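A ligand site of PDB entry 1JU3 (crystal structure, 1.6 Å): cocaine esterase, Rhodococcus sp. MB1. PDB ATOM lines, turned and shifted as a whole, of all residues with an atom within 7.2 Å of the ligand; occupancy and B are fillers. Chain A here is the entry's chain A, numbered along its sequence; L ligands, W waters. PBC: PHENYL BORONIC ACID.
Water W1 lies within hydrogen-bond range of the backbone carbonyl oxygen (O) of Val 116 (3.2 Å) and an oxygen (O1) of the ligand (3.4 Å).
The side-chain hydroxyl of Ser 117 is covalently linked to a boron (B) of the ligand (1.4 Å).
O1 of the ligand lies within hydrogen-bond range of OH of Tyr 44, 2.6 Å away.
The backbone NH of Tyr 118 is in hydrogen-bond range of an oxygen (O1) of the ligand.
NE2 of His 287 lies within hydrogen-bond range of O2 of the ligand (2.6 Å).
Pro 150 touches the ligand (CG to CD1, 3.7 Å).
Trp 151 touches the ligand (CH2 to CD1, 3.6 Å).
NE1 of Trp 166 touches CB1 of the ligand (3.6 Å).
Phe 261 touches the ligand.
Leu 407 touches the ligand (CD1 to CG2, 3.9 Å).
CE2 of Phe 408 touches CG2 of the ligand, at 3.7 Å.
Hydrophobic or aromatic side chains within 4 Å of the ligand: Tyr 44, Tyr 118, Pro 150, Trp 151, Trp 166, Phe 261, His 287, Leu 407 and Phe 408.
Within 4 Å of the ligand: Tyr 44, Ser 117, Tyr 118, Pro 150, Trp 151, Trp 166, Phe 261, His 287, Leu 407 and Phe 408.
The nearest printed residue that does not touch the ligand is Val 116 (4.6 Å).
OH of Tyr 44 sits at hydrogen-bond distance from NE1 of Trp 166, at 2.8 Å.
OG of Ser 117 sits at hydrogen-bond distance from NE2 of His 287, at 2.8 Å.
The side-chain hydroxyl of Tyr 118 lies within hydrogen-bond range of the backbone NH of His 87, 3.2 Å away.
N of Trp 151 is in hydrogen-bond range of O of Leu 146, at 3.4 Å.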
ATOM      1  N   PRO A  43      17.410 -15.652  18.118  1.00  0.00           N
ATOM      2  CA  PRO A  43      16.167 -15.668  18.892  1.00  0.00           C
ATOM      3  C   PRO A  43      15.306 -16.914  18.612  1.00  0.00           C
ATOM      4  O   PRO A  43      14.170 -17.023  19.104  1.00  0.00           O
ATOM      5  CB  PRO A  43      15.457 -14.404  18.421  1.00  0.00           C
ATOM      6  CG  PRO A  43      15.789 -14.377  16.983  1.00  0.00           C
ATOM      7  CD  PRO A  43      17.260 -14.746  16.952  1.00  0.00           C
ATOM      8  N   TYR A  44      15.847 -17.838  17.814  1.00  0.00           N
ATOM      9  CA  TYR A  44      15.146 -19.071  17.408  1.00  0.00           C
ATOM     10  C   TYR A  44      15.815 -20.354  17.916  1.00  0.00           C
ATOM     11  O   TYR A  44      15.811 -21.371  17.206  1.00  0.00           O
ATOM     12  CB  TYR A  44      15.041 -19.140  15.876  1.00  0.00           C
ATOM     13  CG  TYR A  44      14.653 -17.864  15.160  1.00  0.00           C
ATOM     14  CD1 TYR A  44      13.354 -17.324  15.273  1.00  0.00           C
ATOM     15  CD2 TYR A  44      15.588 -17.191  14.334  1.00  0.00           C
ATOM     16  CE1 TYR A  44      12.997 -16.132  14.585  1.00  0.00           C
ATOM     17  CE2 TYR A  44      15.242 -16.006  13.640  1.00  0.00           C
ATOM     18  CZ  TYR A  44      13.938 -15.484  13.770  1.00  0.00           C
ATOM     19  OH  TYR A  44      13.606 -14.334  13.114  1.00  0.00           O
ATOM     20  N   GLN A  55      20.847 -21.179   5.247  1.00  0.00           N
ATOM     21  CA  GLN A  55      20.656 -19.880   4.608  1.00  0.00           C
ATOM     22  C   GLN A  55      21.862 -18.986   4.888  1.00  0.00           C
ATOM     23  O   GLN A  55      21.824 -17.775   4.625  1.00  0.00           O
ATOM     24  CB  GLN A  55      19.396 -19.174   5.133  1.00  0.00           C
ATOM     25  CG  GLN A  55      18.088 -19.936   4.929  1.00  0.00           C
ATOM     26  CD  GLN A  55      17.517 -20.435   6.237  1.00  0.00           C
ATOM     27  OE1 GLN A  55      17.037 -19.653   7.055  1.00  0.00           O
ATOM     28  NE2 GLN A  55      17.582 -21.741   6.446  1.00  0.00           N
ATOM     29  N   HIS A  87      14.423  -6.104  19.381  1.00  0.00           N
ATOM     30  CA  HIS A  87      15.372  -4.999  19.136  1.00  0.00           C
ATOM     31  C   HIS A  87      15.946  -4.142  20.272  1.00  0.00           C
ATOM     32  O   HIS A  87      17.149  -3.872  20.271  1.00  0.00           O
ATOM     33  CB  HIS A  87      14.855  -4.077  18.019  1.00  0.00           C
ATOM     34  CG  HIS A  87      14.267  -4.789  16.841  1.00  0.00           C
ATOM     35  ND1 HIS A  87      12.980  -4.564  16.409  1.00  0.00           N
ATOM     36  CD2 HIS A  87      14.767  -5.763  16.047  1.00  0.00           C
ATOM     37  CE1 HIS A  87      12.717  -5.357  15.389  1.00  0.00           C
ATOM     38  NE2 HIS A  87      13.780  -6.098  15.145  1.00  0.00           N
ATOM     39  N   VAL A 116      22.139 -14.588   9.299  1.00  0.00           N
ATOM     40  CA  VAL A 116      21.083 -14.130   8.419  1.00  0.00           C
ATOM     41  C   VAL A 116      19.824 -13.618   9.137  1.00  0.00           C
ATOM     42  O   VAL A 116      19.465 -14.117  10.202  1.00  0.00           O
ATOM     43  CB  VAL A 116      20.748 -15.273   7.390  1.00  0.00           C
ATOM     44  CG1 VAL A 116      20.139 -16.490   8.096  1.00  0.00           C
ATOM     45  CG2 VAL A 116      19.860 -14.770   6.251  1.00  0.00           C
ATOM     46  N   SER A 117      19.186 -12.622   8.517  1.00  0.00           N
ATOM     47  CA  SER A 117      17.936 -12.024   8.990  1.00  0.00           C
ATOM     48  C   SER A 117      18.062 -11.312  10.345  1.00  0.00           C
ATOM     49  O   SER A 117      18.778 -10.322  10.439  1.00  0.00           O
ATOM     50  CB  SER A 117      16.835 -13.080   8.985  1.00  0.00           C
ATOM     51  OG  SER A 117      15.556 -12.437   9.087  1.00  0.00           O
ATOM     52  N   TYR A 118      17.389 -11.817  11.393  1.00  0.00           N
ATOM     53  CA  TYR A 118      17.483 -11.222  12.736  1.00  0.00           C
ATOM     54  C   TYR A 118      18.931 -11.395  13.243  1.00  0.00           C
ATOM     55  O   TYR A 118      19.441 -10.561  13.981  1.00  0.00           O
ATOM     56  CB  TYR A 118      16.498 -11.860  13.708  1.00  0.00           C
ATOM     57  CG  TYR A 118      16.205 -11.057  14.966  1.00  0.00           C
ATOM     58  CD1 TYR A 118      17.056 -11.133  16.106  1.00  0.00           C
ATOM     59  CD2 TYR A 118      15.050 -10.257  15.060  1.00  0.00           C
ATOM     60  CE1 TYR A 118      16.742 -10.449  17.305  1.00  0.00           C
ATOM     61  CE2 TYR A 118      14.726  -9.566  16.264  1.00  0.00           C
ATOM     62  CZ  TYR A 118      15.578  -9.675  17.380  1.00  0.00           C
ATOM     63  OH  TYR A 118      15.276  -9.033  18.549  1.00  0.00           O
ATOM     64  N   LEU A 119      19.570 -12.476  12.789  1.00  0.00           N
ATOM     65  CA  LEU A 119      20.961 -12.789  13.140  1.00  0.00           C
ATOM     66  C   LEU A 119      21.913 -11.875  12.365  1.00  0.00           C
ATOM     67  O   LEU A 119      23.130 -11.910  12.567  1.00  0.00           O
ATOM     68  CB  LEU A 119      21.274 -14.253  12.831  1.00  0.00           C
ATOM     69  CG  LEU A 119      20.651 -15.371  13.665  1.00  0.00           C
ATOM     70  CD1 LEU A 119      19.130 -15.390  13.655  1.00  0.00           C
ATOM     71  CD2 LEU A 119      21.153 -16.647  13.122  1.00  0.00           C
ATOM     72  N   GLY A 120      21.329 -11.095  11.455  1.00  0.00           N
ATOM     73  CA  GLY A 120      22.071 -10.123  10.668  1.00  0.00           C
ATOM     74  C   GLY A 120      21.849  -8.746  11.251  1.00  0.00           C
ATOM     75  O   GLY A 120      22.788  -7.948  11.347  1.00  0.00           O
ATOM     76  N   VAL A 121      20.610  -8.444  11.656  1.00  0.00           N
ATOM     77  CA  VAL A 121      20.244  -7.157  12.266  1.00  0.00           C
ATOM     78  C   VAL A 121      21.039  -6.933  13.562  1.00  0.00           C
ATOM     79  O   VAL A 121      21.546  -5.830  13.807  1.00  0.00           O
ATOM     80  CB  VAL A 121      18.700  -7.078  12.550  1.00  0.00           C
ATOM     81  CG1 VAL A 121      18.323  -5.834  13.377  1.00  0.00           C
ATOM     82  CG2 VAL A 121      17.930  -7.065  11.235  1.00  0.00           C
ATOM     83  N   MET A 141      20.840 -10.583   4.488  1.00  0.00           N
ATOM     84  CA  MET A 141      19.402 -10.255   4.386  1.00  0.00           C
ATOM     85  C   MET A 141      18.943  -9.473   5.626  1.00  0.00           C
ATOM     86  O   MET A 141      17.971  -9.822   6.305  1.00  0.00           O
ATOM     87  CB  MET A 141      18.603 -11.542   4.174  1.00  0.00           C
ATOM     88  CG  MET A 141      18.911 -12.219   2.847  1.00  0.00           C
ATOM     89  SD  MET A 141      18.058 -13.793   2.665  1.00  0.00           S
ATOM     90  CE  MET A 141      19.456 -14.842   2.362  1.00  0.00           C
ATOM     91  N   LEU A 146      15.096  -0.427  11.233  1.00  0.00           N
ATOM     92  CA  LEU A 146      13.935  -1.286  11.426  1.00  0.00           C
ATOM     93  C   LEU A 146      12.589  -0.782  10.903  1.00  0.00           C
ATOM     94  O   LEU A 146      11.728  -1.593  10.561  1.00  0.00           O
ATOM     95  CB  LEU A 146      13.835  -1.760  12.881  1.00  0.00           C
ATOM     96  CG  LEU A 146      14.905  -2.726  13.408  1.00  0.00           C
ATOM     97  CD1 LEU A 146      15.101  -3.907  12.455  1.00  0.00           C
ATOM     98  CD2 LEU A 146      16.224  -2.017  13.667  1.00  0.00           C
ATOM     99  N   PRO A 150      12.192  -4.492   8.418  1.00  0.00           N
ATOM    100  CA  PRO A 150      11.040  -5.033   7.693  1.00  0.00           C
ATOM    101  C   PRO A 150       9.636  -4.582   8.087  1.00  0.00           C
ATOM    102  O   PRO A 150       8.667  -5.000   7.457  1.00  0.00           O
ATOM    103  CB  PRO A 150      11.186  -6.522   7.979  1.00  0.00           C
ATOM    104  CG  PRO A 150      11.558  -6.510   9.453  1.00  0.00           C
ATOM    105  CD  PRO A 150      12.478  -5.303   9.627  1.00  0.00           C
ATOM    106  N   TRP A 151       9.532  -3.717   9.099  1.00  0.00           N
ATOM    107  CA  TRP A 151       8.219  -3.317   9.593  1.00  0.00           C
ATOM    108  C   TRP A 151       7.350  -2.368   8.809  1.00  0.00           C
ATOM    109  O   TRP A 151       6.135  -2.586   8.701  1.00  0.00           O
ATOM    110  CB  TRP A 151       8.292  -2.956  11.087  1.00  0.00           C
ATOM    111  CG  TRP A 151       9.071  -3.969  11.926  1.00  0.00           C
ATOM    112  CD1 TRP A 151      10.116  -3.687  12.760  1.00  0.00           C
ATOM    113  CD2 TRP A 151       8.926  -5.406  11.946  1.00  0.00           C
ATOM    114  NE1 TRP A 151      10.631  -4.834  13.292  1.00  0.00           N
ATOM    115  CE2 TRP A 151       9.934  -5.904  12.803  1.00  0.00           C
ATOM    116  CE3 TRP A 151       8.057  -6.318  11.308  1.00  0.00           C
ATOM    117  CZ2 TRP A 151      10.103  -7.287  13.044  1.00  0.00           C
ATOM    118  CZ3 TRP A 151       8.225  -7.701  11.549  1.00  0.00           C
ATOM    119  CH2 TRP A 151       9.239  -8.160  12.418  1.00  0.00           C
ATOM    120  N   ALA A 162       4.468  -9.019   7.142  1.00  0.00           N
ATOM    121  CA  ALA A 162       5.764  -9.230   7.785  1.00  0.00           C
ATOM    122  C   ALA A 162       5.575  -9.227   9.295  1.00  0.00           C
ATOM    123  O   ALA A 162       6.071 -10.103   9.985  1.00  0.00           O
ATOM    124  CB  ALA A 162       6.737  -8.147   7.383  1.00  0.00           C
ATOM    125  N   LEU A 163       4.795  -8.255   9.768  1.00  0.00           N
ATOM    126  CA  LEU A 163       4.523  -8.111  11.197  1.00  0.00           C
ATOM    127  C   LEU A 163       3.761  -9.275  11.809  1.00  0.00           C
ATOM    128  O   LEU A 163       4.238  -9.871  12.771  1.00  0.00           O
ATOM    129  CB  LEU A 163       3.807  -6.789  11.485  1.00  0.00           C
ATOM    130  CG  LEU A 163       3.483  -6.532  12.969  1.00  0.00           C
ATOM    131  CD1 LEU A 163       4.766  -6.378  13.782  1.00  0.00           C
ATOM    132  CD2 LEU A 163       2.591  -5.328  13.096  1.00  0.00           C
ATOM    133  N   GLY A 165       3.132 -12.269  10.492  1.00  0.00           N
ATOM    134  CA  GLY A 165       3.794 -13.544  10.236  1.00  0.00           C
ATOM    135  C   GLY A 165       4.941 -13.805  11.186  1.00  0.00           C
ATOM    136  O   GLY A 165       5.020 -14.883  11.781  1.00  0.00           O
ATOM    137  N   TRP A 166       5.802 -12.809  11.386  1.00  0.00           N
ATOM    138  CA  TRP A 166       6.948 -12.950  12.280  1.00  0.00           C
ATOM    139  C   TRP A 166       6.519 -13.041  13.743  1.00  0.00           C
ATOM    140  O   TRP A 166       7.122 -13.798  14.514  1.00  0.00           O
ATOM    141  CB  TRP A 166       7.947 -11.806  12.114  1.00  0.00           C
ATOM    142  CG  TRP A 166       9.243 -12.032  12.850  1.00  0.00           C
ATOM    143  CD1 TRP A 166      10.267 -12.868  12.483  1.00  0.00           C
ATOM    144  CD2 TRP A 166       9.660 -11.409  14.074  1.00  0.00           C
ATOM    145  NE1 TRP A 166      11.300 -12.785  13.379  1.00  0.00           N
ATOM    146  CE2 TRP A 166      10.957 -11.892  14.366  1.00  0.00           C
ATOM    147  CE3 TRP A 166       9.050 -10.488  14.944  1.00  0.00           C
ATOM    148  CZ2 TRP A 166      11.678 -11.485  15.507  1.00  0.00           C
ATOM    149  CZ3 TRP A 166       9.769 -10.063  16.092  1.00  0.00           C
ATOM    150  CH2 TRP A 166      11.075 -10.574  16.350  1.00  0.00           C
ATOM    151  N   LEU A 169       5.427 -16.446  14.417  1.00  0.00           N
ATOM    152  CA  LEU A 169       6.574 -17.357  14.439  1.00  0.00           C
ATOM    153  C   LEU A 169       7.255 -17.273  15.813  1.00  0.00           C
ATOM    154  O   LEU A 169       7.605 -18.301  16.410  1.00  0.00           O
ATOM    155  CB  LEU A 169       7.565 -17.018  13.323  1.00  0.00           C
ATOM    156  CG  LEU A 169       8.838 -17.870  13.147  1.00  0.00           C
ATOM    157  CD1 LEU A 169       8.486 -19.262  12.635  1.00  0.00           C
ATOM    158  CD2 LEU A 169       9.780 -17.172  12.175  1.00  0.00           C
ATOM    159  N   PHE A 261      14.235  -7.291   2.931  1.00  0.00           N
ATOM    160  CA  PHE A 261      15.264  -6.406   3.463  1.00  0.00           C
ATOM    161  C   PHE A 261      16.212  -5.834   2.400  1.00  0.00           C
ATOM    162  O   PHE A 261      17.078  -5.038   2.756  1.00  0.00           O
ATOM    163  CB  PHE A 261      16.142  -7.145   4.485  1.00  0.00           C
ATOM    164  CG  PHE A 261      15.421  -7.650   5.710  1.00  0.00           C
ATOM    165  CD1 PHE A 261      14.591  -8.780   5.640  1.00  0.00           C
ATOM    166  CD2 PHE A 261      15.650  -7.054   6.952  1.00  0.00           C
ATOM    167  CE1 PHE A 261      13.991  -9.318   6.820  1.00  0.00           C
ATOM    168  CE2 PHE A 261      15.079  -7.578   8.130  1.00  0.00           C
ATOM    169  CZ  PHE A 261      14.242  -8.723   8.067  1.00  0.00           C
ATOM    170  N   HIS A 287      13.238 -14.265   1.008  1.00  0.00           N
ATOM    171  CA  HIS A 287      13.619 -14.650   2.368  1.00  0.00           C
ATOM    172  C   HIS A 287      13.496 -16.128   2.718  1.00  0.00           C
ATOM    173  O   HIS A 287      14.381 -16.696   3.362  1.00  0.00           O
ATOM    174  CB  HIS A 287      12.829 -13.826   3.382  1.00  0.00           C
ATOM    175  CG  HIS A 287      13.590 -13.476   4.624  1.00  0.00           C
ATOM    176  ND1 HIS A 287      14.649 -12.594   4.620  1.00  0.00           N
ATOM    177  CD2 HIS A 287      13.433 -13.880   5.912  1.00  0.00           C
ATOM    178  CE1 HIS A 287      15.116 -12.465   5.848  1.00  0.00           C
ATOM    179  NE2 HIS A 287      14.401 -13.233   6.647  1.00  0.00           N
ATOM    180  N   LEU A 407       7.419 -11.533   2.691  1.00  0.00           N
ATOM    181  CA  LEU A 407       8.191 -12.316   3.660  1.00  0.00           C
ATOM    182  C   LEU A 407       7.521 -13.605   4.147  1.00  0.00           C
ATOM    183  O   LEU A 407       8.110 -14.682   4.026  1.00  0.00           O
ATOM    184  CB  LEU A 407       8.575 -11.437   4.854  1.00  0.00           C
ATOM    185  CG  LEU A 407       9.595 -10.308   4.621  1.00  0.00           C
ATOM    186  CD1 LEU A 407       9.758  -9.471   5.859  1.00  0.00           C
ATOM    187  CD2 LEU A 407      10.934 -10.884   4.254  1.00  0.00           C
ATOM    188  N   PHE A 408       6.297 -13.488   4.668  1.00  0.00           N
ATOM    189  CA  PHE A 408       5.558 -14.630   5.205  1.00  0.00           C
ATOM    190  C   PHE A 408       4.354 -15.083   4.405  1.00  0.00           C
ATOM    191  O   PHE A 408       4.068 -16.290   4.349  1.00  0.00           O
ATOM    192  CB  PHE A 408       5.164 -14.367   6.655  1.00  0.00           C
ATOM    193  CG  PHE A 408       6.321 -14.437   7.617  1.00  0.00           C
ATOM    194  CD1 PHE A 408       6.639 -15.662   8.239  1.00  0.00           C
ATOM    195  CD2 PHE A 408       7.132 -13.316   7.843  1.00  0.00           C
ATOM    196  CE1 PHE A 408       7.782 -15.776   9.089  1.00  0.00           C
ATOM    197  CE2 PHE A 408       8.277 -13.403   8.681  1.00  0.00           C
ATOM    198  CZ  PHE A 408       8.599 -14.640   9.308  1.00  0.00           C
HETATM  199  B   PBC L   1      14.445 -13.087   9.726  1.00  0.00           B
HETATM  200  O1  PBC L   1      14.942 -13.521  10.994  1.00  0.00           O
HETATM  201  O2  PBC L   1      14.097 -14.276   9.057  1.00  0.00           O
HETATM  202  CG1 PBC L   1      12.270 -10.159  11.106  1.00  0.00           C
HETATM  203  CD1 PBC L   1      11.197 -10.160  10.183  1.00  0.00           C
HETATM  204  CG2 PBC L   1      11.152 -11.101   9.129  1.00  0.00           C
HETATM  205  CB2 PBC L   1      12.198 -12.042   8.981  1.00  0.00           C
HETATM  206  CA  PBC L   1      13.285 -12.061   9.903  1.00  0.00           C
HETATM  207  CB1 PBC L   1      13.319 -11.104  10.966  1.00  0.00           C
HETATM  208  O   HOH W   1      17.049 -16.181  10.673  1.00  0.00           O
HETATM  209  O   HOH W   2      15.765 -16.343   7.544  1.00  0.00           O
HETATM  210  O   HOH W   3      12.017 -15.552   9.813  1.00  0.00           O
